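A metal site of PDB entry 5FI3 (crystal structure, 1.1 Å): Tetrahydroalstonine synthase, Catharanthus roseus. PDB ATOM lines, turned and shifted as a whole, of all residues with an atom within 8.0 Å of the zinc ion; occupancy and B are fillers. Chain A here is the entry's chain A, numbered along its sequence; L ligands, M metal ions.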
ATOM      1  N   GLY A  53       2.512 -25.411 -15.631  1.00  0.00           N
ATOM      2  CA  GLY A  53       2.069 -25.089 -14.292  1.00  0.00           C
ATOM      3  C   GLY A  53       1.817 -23.615 -14.189  1.00  0.00           C
ATOM      4  O   GLY A  53       2.440 -22.810 -14.889  1.00  0.00           O
ATOM      5  N   THR A  54       0.929 -23.227 -13.288  1.00  0.00           N
ATOM      6  CA  THR A  54       0.805 -21.808 -12.950  1.00  0.00           C
ATOM      7  C   THR A  54       0.725 -21.678 -11.445  1.00  0.00           C
ATOM      8  O   THR A  54       0.669 -22.678 -10.708  1.00  0.00           O
ATOM      9  CB  THR A  54      -0.327 -21.126 -13.711  1.00  0.00           C
ATOM     10  OG1 THR A  54      -0.251 -19.703 -13.545  1.00  0.00           O
ATOM     11  CG2 THR A  54      -1.704 -21.640 -13.282  1.00  0.00           C
ATOM     12  N   CYS A  55       0.762 -20.434 -10.990  1.00  0.00           N
ATOM     13  CA  CYS A  55       1.004 -20.204  -9.576  1.00  0.00           C
ATOM     14  C   CYS A  55       0.784 -18.754  -9.239  1.00  0.00           C
ATOM     15  O   CYS A  55       0.520 -17.917 -10.129  1.00  0.00           O
ATOM     16  CB  CYS A  55       2.431 -20.645  -9.210  1.00  0.00           C
ATOM     17  SG  CYS A  55       3.697 -19.557  -9.895  1.00  0.00           S
ATOM     18  N   GLN A  56       0.907 -18.446  -7.954  1.00  0.00           N
ATOM     19  CA  GLN A  56       0.689 -17.099  -7.467  1.00  0.00           C
ATOM     20  C   GLN A  56       1.539 -16.085  -8.200  1.00  0.00           C
ATOM     21  O   GLN A  56       1.092 -14.984  -8.443  1.00  0.00           O
ATOM     22  CB  GLN A  56       0.925 -17.038  -5.959  1.00  0.00           C
ATOM     23  CG  GLN A  56       0.480 -15.770  -5.289  1.00  0.00           C
ATOM     24  CD  GLN A  56      -1.007 -15.555  -5.430  1.00  0.00           C
ATOM     25  OE1 GLN A  56      -1.435 -14.639  -6.104  1.00  0.00           O
ATOM     26  NE2 GLN A  56      -1.793 -16.426  -4.829  1.00  0.00           N
ATOM     27  N   TYR A  57       2.784 -16.421  -8.526  1.00  0.00           N
ATOM     28  CA  TYR A  57       3.657 -15.513  -9.235  1.00  0.00           C
ATOM     29  C   TYR A  57       3.048 -15.041 -10.543  1.00  0.00           C
ATOM     30  O   TYR A  57       3.149 -13.873 -10.915  1.00  0.00           O
ATOM     31  CB  TYR A  57       5.016 -16.142  -9.503  1.00  0.00           C
ATOM     32  CG  TYR A  57       5.994 -15.232 -10.189  1.00  0.00           C
ATOM     33  CD1 TYR A  57       6.736 -14.298  -9.459  1.00  0.00           C
ATOM     34  CD2 TYR A  57       6.206 -15.313 -11.554  1.00  0.00           C
ATOM     35  CE1 TYR A  57       7.654 -13.477 -10.069  1.00  0.00           C
ATOM     36  CE2 TYR A  57       7.122 -14.473 -12.180  1.00  0.00           C
ATOM     37  CZ  TYR A  57       7.850 -13.569 -11.420  1.00  0.00           C
ATOM     38  OH  TYR A  57       8.766 -12.751 -12.021  1.00  0.00           O
ATOM     39  N   ASP A  58       2.369 -15.950 -11.273  1.00  0.00           N
ATOM     40  CA  ASP A  58       1.687 -15.509 -12.499  1.00  0.00           C
ATOM     41  C   ASP A  58       0.560 -14.528 -12.228  1.00  0.00           C
ATOM     42  O   ASP A  58       0.393 -13.593 -12.991  1.00  0.00           O
ATOM     43  CB  ASP A  58       1.145 -16.684 -13.318  1.00  0.00           C
ATOM     44  CG  ASP A  58       2.218 -17.439 -14.063  1.00  0.00           C
ATOM     45  OD1 ASP A  58       3.174 -16.835 -14.552  1.00  0.00           O
ATOM     46  OD2 ASP A  58       2.088 -18.619 -14.205  1.00  0.00           O
ATOM     47  N   GLY A  76       3.744 -18.367 -18.104  1.00  0.00           N
ATOM     48  CA  GLY A  76       4.194 -19.739 -18.227  1.00  0.00           C
ATOM     49  C   GLY A  76       5.687 -19.919 -18.009  1.00  0.00           C
ATOM     50  O   GLY A  76       6.500 -19.782 -18.960  1.00  0.00           O
ATOM     51  N   HIS A  77       6.037 -20.243 -16.784  1.00  0.00           N
ATOM     52  CA  HIS A  77       7.442 -20.339 -16.450  1.00  0.00           C
ATOM     53  C   HIS A  77       7.812 -21.681 -15.873  1.00  0.00           C
ATOM     54  O   HIS A  77       8.929 -21.820 -15.368  1.00  0.00           O
ATOM     55  CB  HIS A  77       7.841 -19.196 -15.490  1.00  0.00           C
ATOM     56  CG  HIS A  77       7.053 -19.230 -14.221  1.00  0.00           C
ATOM     57  ND1 HIS A  77       5.952 -18.440 -14.029  1.00  0.00           N
ATOM     58  CD2 HIS A  77       7.125 -20.047 -13.140  1.00  0.00           C
ATOM     59  CE1 HIS A  77       5.364 -18.788 -12.894  1.00  0.00           C
ATOM     60  NE2 HIS A  77       6.039 -19.760 -12.335  1.00  0.00           N
ATOM     61  N   GLU A  78       6.937 -22.670 -15.984  1.00  0.00           N
ATOM     62  CA  GLU A  78       7.152 -24.012 -15.451  1.00  0.00           C
ATOM     63  C   GLU A  78       6.451 -24.957 -16.412  1.00  0.00           C
ATOM     64  O   GLU A  78       5.223 -24.996 -16.430  1.00  0.00           O
ATOM     65  CB  GLU A  78       6.696 -24.162 -13.956  1.00  0.00           C
ATOM     66  CG  GLU A  78       5.580 -23.231 -13.538  1.00  0.00           C
ATOM     67  CD  GLU A  78       4.854 -23.564 -12.246  1.00  0.00           C
ATOM     68  OE1 GLU A  78       4.515 -24.721 -12.018  1.00  0.00           O
ATOM     69  OE2 GLU A  78       4.561 -22.588 -11.466  1.00  0.00           O
ATOM     70  N   SER A 103      12.222 -21.364 -14.891  1.00  0.00           N
ATOM     71  CA  SER A 103      11.978 -19.980 -15.192  1.00  0.00           C
ATOM     72  C   SER A 103      13.116 -19.247 -15.869  1.00  0.00           C
ATOM     73  O   SER A 103      12.861 -18.250 -16.490  1.00  0.00           O
ATOM     74  CB  SER A 103      11.564 -19.216 -13.949  1.00  0.00           C
ATOM     75  OG  SER A 103      12.627 -19.066 -13.050  1.00  0.00           O
ATOM     76  N   VAL A 159       5.096 -31.145 -12.937  1.00  0.00           N
ATOM     77  CA  VAL A 159       5.569 -29.889 -13.523  1.00  0.00           C
ATOM     78  C   VAL A 159       5.803 -28.796 -12.474  1.00  0.00           C
ATOM     79  O   VAL A 159       6.760 -28.037 -12.614  1.00  0.00           O
ATOM     80  CB  VAL A 159       4.714 -29.422 -14.734  1.00  0.00           C
ATOM     81  CG1 VAL A 159       3.265 -29.148 -14.398  1.00  0.00           C
ATOM     82  CG2 VAL A 159       5.329 -28.207 -15.389  1.00  0.00           C
ATOM     83  N   PRO A 160       4.993 -28.674 -11.385  1.00  0.00           N
ATOM     84  CA  PRO A 160       5.300 -27.612 -10.428  1.00  0.00           C
ATOM     85  C   PRO A 160       6.624 -27.794  -9.699  1.00  0.00           C
ATOM     86  O   PRO A 160       7.091 -26.822  -9.070  1.00  0.00           O
ATOM     87  CB  PRO A 160       4.122 -27.682  -9.437  1.00  0.00           C
ATOM     88  CG  PRO A 160       3.027 -28.314 -10.251  1.00  0.00           C
ATOM     89  CD  PRO A 160       3.743 -29.364 -11.040  1.00  0.00           C
ATOM     90  N   LEU A 162       9.286 -27.681 -11.089  1.00  0.00           N
ATOM     91  CA  LEU A 162      10.151 -26.736 -11.799  1.00  0.00           C
ATOM     92  C   LEU A 162      10.000 -25.296 -11.321  1.00  0.00           C
ATOM     93  O   LEU A 162      10.738 -24.430 -11.783  1.00  0.00           O
ATOM     94  CB  LEU A 162       9.886 -26.814 -13.297  1.00  0.00           C
ATOM     95  CG  LEU A 162      10.260 -28.153 -13.930  1.00  0.00           C
ATOM     96  CD1 LEU A 162       9.574 -28.287 -15.258  1.00  0.00           C
ATOM     97  CD2 LEU A 162      11.762 -28.236 -14.108  1.00  0.00           C
ATOM     98  N   CYS A 163       9.084 -25.039 -10.403  1.00  0.00           N
ATOM     99  CA  CYS A 163       8.852 -23.727  -9.791  1.00  0.00           C
ATOM    100  C   CYS A 163       8.955 -23.918  -8.275  1.00  0.00           C
ATOM    101  O   CYS A 163       9.969 -23.538  -7.667  1.00  0.00           O
ATOM    102  CB  CYS A 163       7.520 -23.162 -10.236  1.00  0.00           C
ATOM    103  SG  CYS A 163       7.053 -21.617  -9.427  1.00  0.00           S
ATOM    104  N   ALA A 164       7.961 -24.534  -7.669  1.00  0.00           N
ATOM    105  CA  ALA A 164       7.984 -24.761  -6.225  1.00  0.00           C
ATOM    106  C   ALA A 164       9.137 -25.682  -5.784  1.00  0.00           C
ATOM    107  O   ALA A 164       9.748 -25.446  -4.739  1.00  0.00           O
ATOM    108  CB  ALA A 164       6.670 -25.308  -5.793  1.00  0.00           C
ATOM    109  N   THR A 167      12.586 -23.919  -6.051  1.00  0.00           N
ATOM    110  CA  THR A 167      12.652 -22.743  -5.161  1.00  0.00           C
ATOM    111  C   THR A 167      12.852 -23.160  -3.720  1.00  0.00           C
ATOM    112  O   THR A 167      13.560 -22.466  -2.978  1.00  0.00           O
ATOM    113  CB  THR A 167      11.426 -21.875  -5.378  1.00  0.00           C
ATOM    114  OG1 THR A 167      11.456 -21.355  -6.727  1.00  0.00           O
ATOM    115  CG2 THR A 167      11.367 -20.704  -4.432  1.00  0.00           C
ATOM    116  N   ARG A 345      -1.955 -26.583  -6.539  1.00  0.00           N
ATOM    117  CA  ARG A 345      -1.449 -25.879  -7.715  1.00  0.00           C
ATOM    118  C   ARG A 345      -2.360 -26.152  -8.879  1.00  0.00           C
ATOM    119  O   ARG A 345      -2.772 -27.295  -9.058  1.00  0.00           O
ATOM    120  CB  ARG A 345      -0.083 -26.444  -8.154  1.00  0.00           C
ATOM    121  CG  ARG A 345       0.947 -26.425  -7.069  1.00  0.00           C
ATOM    122  CD  ARG A 345       1.526 -25.031  -6.922  1.00  0.00           C
ATOM    123  NE  ARG A 345       2.521 -24.704  -7.933  1.00  0.00           N
ATOM    124  CZ  ARG A 345       3.542 -23.878  -7.726  1.00  0.00           C
ATOM    125  NH1 ARG A 345       3.690 -23.256  -6.548  1.00  0.00           N
ATOM    126  NH2 ARG A 345       4.429 -23.653  -8.675  1.00  0.00           N
ATOM    127  N   PHE A 346      -2.568 -25.136  -9.699  1.00  0.00           N
ATOM    128  CA  PHE A 346      -3.188 -25.322 -11.007  1.00  0.00           C
ATOM    129  C   PHE A 346      -2.150 -25.684 -12.040  1.00  0.00           C
ATOM    130  O   PHE A 346      -1.061 -25.099 -12.100  1.00  0.00           O
ATOM    131  CB  PHE A 346      -3.839 -24.010 -11.450  1.00  0.00           C
ATOM    132  CG  PHE A 346      -5.058 -23.622 -10.652  1.00  0.00           C
ATOM    133  CD1 PHE A 346      -6.213 -24.390 -10.698  1.00  0.00           C
ATOM    134  CD2 PHE A 346      -5.059 -22.479  -9.852  1.00  0.00           C
ATOM    135  CE1 PHE A 346      -7.338 -24.005  -9.998  1.00  0.00           C
ATOM    136  CE2 PHE A 346      -6.183 -22.117  -9.149  1.00  0.00           C
ATOM    137  CZ  PHE A 346      -7.327 -22.865  -9.229  1.00  0.00           C
HETATM  138  P1  LIG L   1       0.021 -19.381  -2.653  1.00  0.00           P
HETATM  139  O1  LIG L   1      -0.988 -18.274  -2.800  1.00  0.00           O
HETATM  140  O2  LIG L   1      -0.248 -20.709  -3.335  1.00  0.00           O
HETATM  141  O3  LIG L   1       0.346 -19.761  -1.151  1.00  0.00           O
HETATM  142  C1  LIG L   1       0.724 -18.743  -0.225  1.00  0.00           C
HETATM  143  C2  LIG L   1       0.259 -19.191   1.150  1.00  0.00           C
HETATM  144  O4  LIG L   1       0.662 -18.141   2.060  1.00  0.00           O
HETATM  145  C3  LIG L   1      -1.252 -19.261   1.298  1.00  0.00           C
HETATM  146  O5  LIG L   1      -1.815 -20.515   0.953  1.00  0.00           O
HETATM  147  C4  LIG L   1      -1.445 -18.922   2.761  1.00  0.00           C
HETATM  148  O6  LIG L   1      -1.150 -20.088   3.551  1.00  0.00           O
HETATM  149  C5  LIG L   1      -0.349 -17.897   3.028  1.00  0.00           C
HETATM  150  N1  LIG L   1      -0.772 -16.512   2.925  1.00  0.00           N
HETATM  151  C6  LIG L   1      -1.225 -15.845   1.822  1.00  0.00           C
HETATM  152  N2  LIG L   1      -1.450 -14.566   2.028  1.00  0.00           N
HETATM  153  C7  LIG L   1      -1.127 -14.398   3.364  1.00  0.00           C
HETATM  154  C8  LIG L   1      -1.110 -13.258   4.187  1.00  0.00           C
HETATM  155  N3  LIG L   1      -1.492 -12.053   3.767  1.00  0.00           N
HETATM  156  N4  LIG L   1      -0.690 -13.434   5.465  1.00  0.00           N
HETATM  157  C9  LIG L   1      -0.345 -14.650   5.884  1.00  0.00           C
HETATM  158  N5  LIG L   1      -0.321 -15.789   5.198  1.00  0.00           N
HETATM  159  C10 LIG L   1      -0.723 -15.590   3.932  1.00  0.00           C
HETATM  160  O7  LIG L   1       1.393 -18.742  -3.225  1.00  0.00           O
HETATM  161  P2  LIG L   1       2.740 -19.524  -3.609  1.00  0.00           P
HETATM  162  O8  LIG L   1       3.064 -20.465  -2.504  1.00  0.00           O
HETATM  163  O9  LIG L   1       2.613 -20.046  -4.975  1.00  0.00           O
HETATM  164  O10 LIG L   1       3.764 -18.328  -3.721  1.00  0.00           O
HETATM  165  C11 LIG L   1       4.080 -17.621  -2.523  1.00  0.00           C
HETATM  166  C12 LIG L   1       5.030 -16.511  -2.839  1.00  0.00           C
HETATM  167  O11 LIG L   1       6.260 -17.050  -3.319  1.00  0.00           O
HETATM  168  C13 LIG L   1       4.566 -15.497  -3.875  1.00  0.00           C
HETATM  169  O12 LIG L   1       4.844 -14.186  -3.358  1.00  0.00           O
HETATM  170  C14 LIG L   1       5.409 -15.833  -5.102  1.00  0.00           C
HETATM  171  O13 LIG L   1       5.704 -14.726  -5.935  1.00  0.00           O
HETATM  172  C15 LIG L   1       6.680 -16.262  -4.411  1.00  0.00           C
HETATM  173  N6  LIG L   1       7.597 -17.068  -5.271  1.00  0.00           N
HETATM  174  C16 LIG L   1       8.903 -16.825  -5.095  1.00  0.00           C
HETATM  175  C17 LIG L   1       9.833 -17.572  -5.771  1.00  0.00           C
HETATM  176  C18 LIG L   1      11.278 -17.441  -5.452  1.00  0.00           C
HETATM  177  O14 LIG L   1      12.099 -17.842  -6.265  1.00  0.00           O
HETATM  178  N7  LIG L   1      11.625 -16.837  -4.302  1.00  0.00           N
HETATM  179  C19 LIG L   1       9.395 -18.542  -6.684  1.00  0.00           C
HETATM  180  C20 LIG L   1       8.045 -18.781  -6.836  1.00  0.00           C
HETATM  181  C21 LIG L   1       7.147 -18.048  -6.093  1.00  0.00           C
HETATM  182  P3  LIG L   1      -2.130 -20.499   4.763  1.00  0.00           P
HETATM  183  O15 LIG L   1      -1.497 -21.747   5.288  1.00  0.00           O
HETATM  184  O16 LIG L   1      -3.471 -20.692   4.146  1.00  0.00           O
HETATM  185  O17 LIG L   1      -2.139 -19.357   5.744  1.00  0.00           O
HETATM  186 ZN    ZN M   1       5.340 -20.880 -10.799  1.00  0.00          ZN
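The backbone NH (N) of Tyr 57 sits close to the side-chain sulfur (SG) of Cys 55 (3.5 Å). O of Glu 78 lies within hydrogen-bond range of N of Gly 53 (2.9 Å). The side-chain hydroxyl of Thr 167 sits at hydrogen-bond distance from the backbone carbonyl oxygen of Cys 163. The guanidinium group (NH2) of Arg 345 lies close to the side-chain sulfur (SG) of Cys 163 (3.4 Å). OD1 of Asp 58 is in hydrogen-bond range of ND1 of His 77, at 3.3 Å. The backbone carbonyl oxygen (O) of His 77 is in hydrogen-bond range of the backbone NH (N) of Ser 103 (3.4 Å). OE1 of Glu 78 lies within salt-bridge range of NH2 of Arg 345 (3.5 Å).
The zinc ion is bound by the side-chain carboxylate of Glu 78 (2.0 Å), a ring nitrogen (NE2) of His 77 (2.0 Å), the side-chain sulfur of Cys 55 (2.3 Å) and the side-chain sulfur of Cys 163 (2.3 Å).
The guanidinium group (NH1) of Arg 345 lies within salt-bridge range of an oxygen (O9) of the ligand (3.7 Å). The side-chain amide nitrogen (NE2) of Gln 56 is in hydrogen-bond range of an oxygen (O1) of the ligand (2.9 Å).
Merely in contact with the zinc ion: Arg 345. Along chain A the residues within 4 Å of the zinc ion span positions 55 to 345. The nearest printed residue that does not touch the zinc ion is Thr 54 (4.7 Å).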
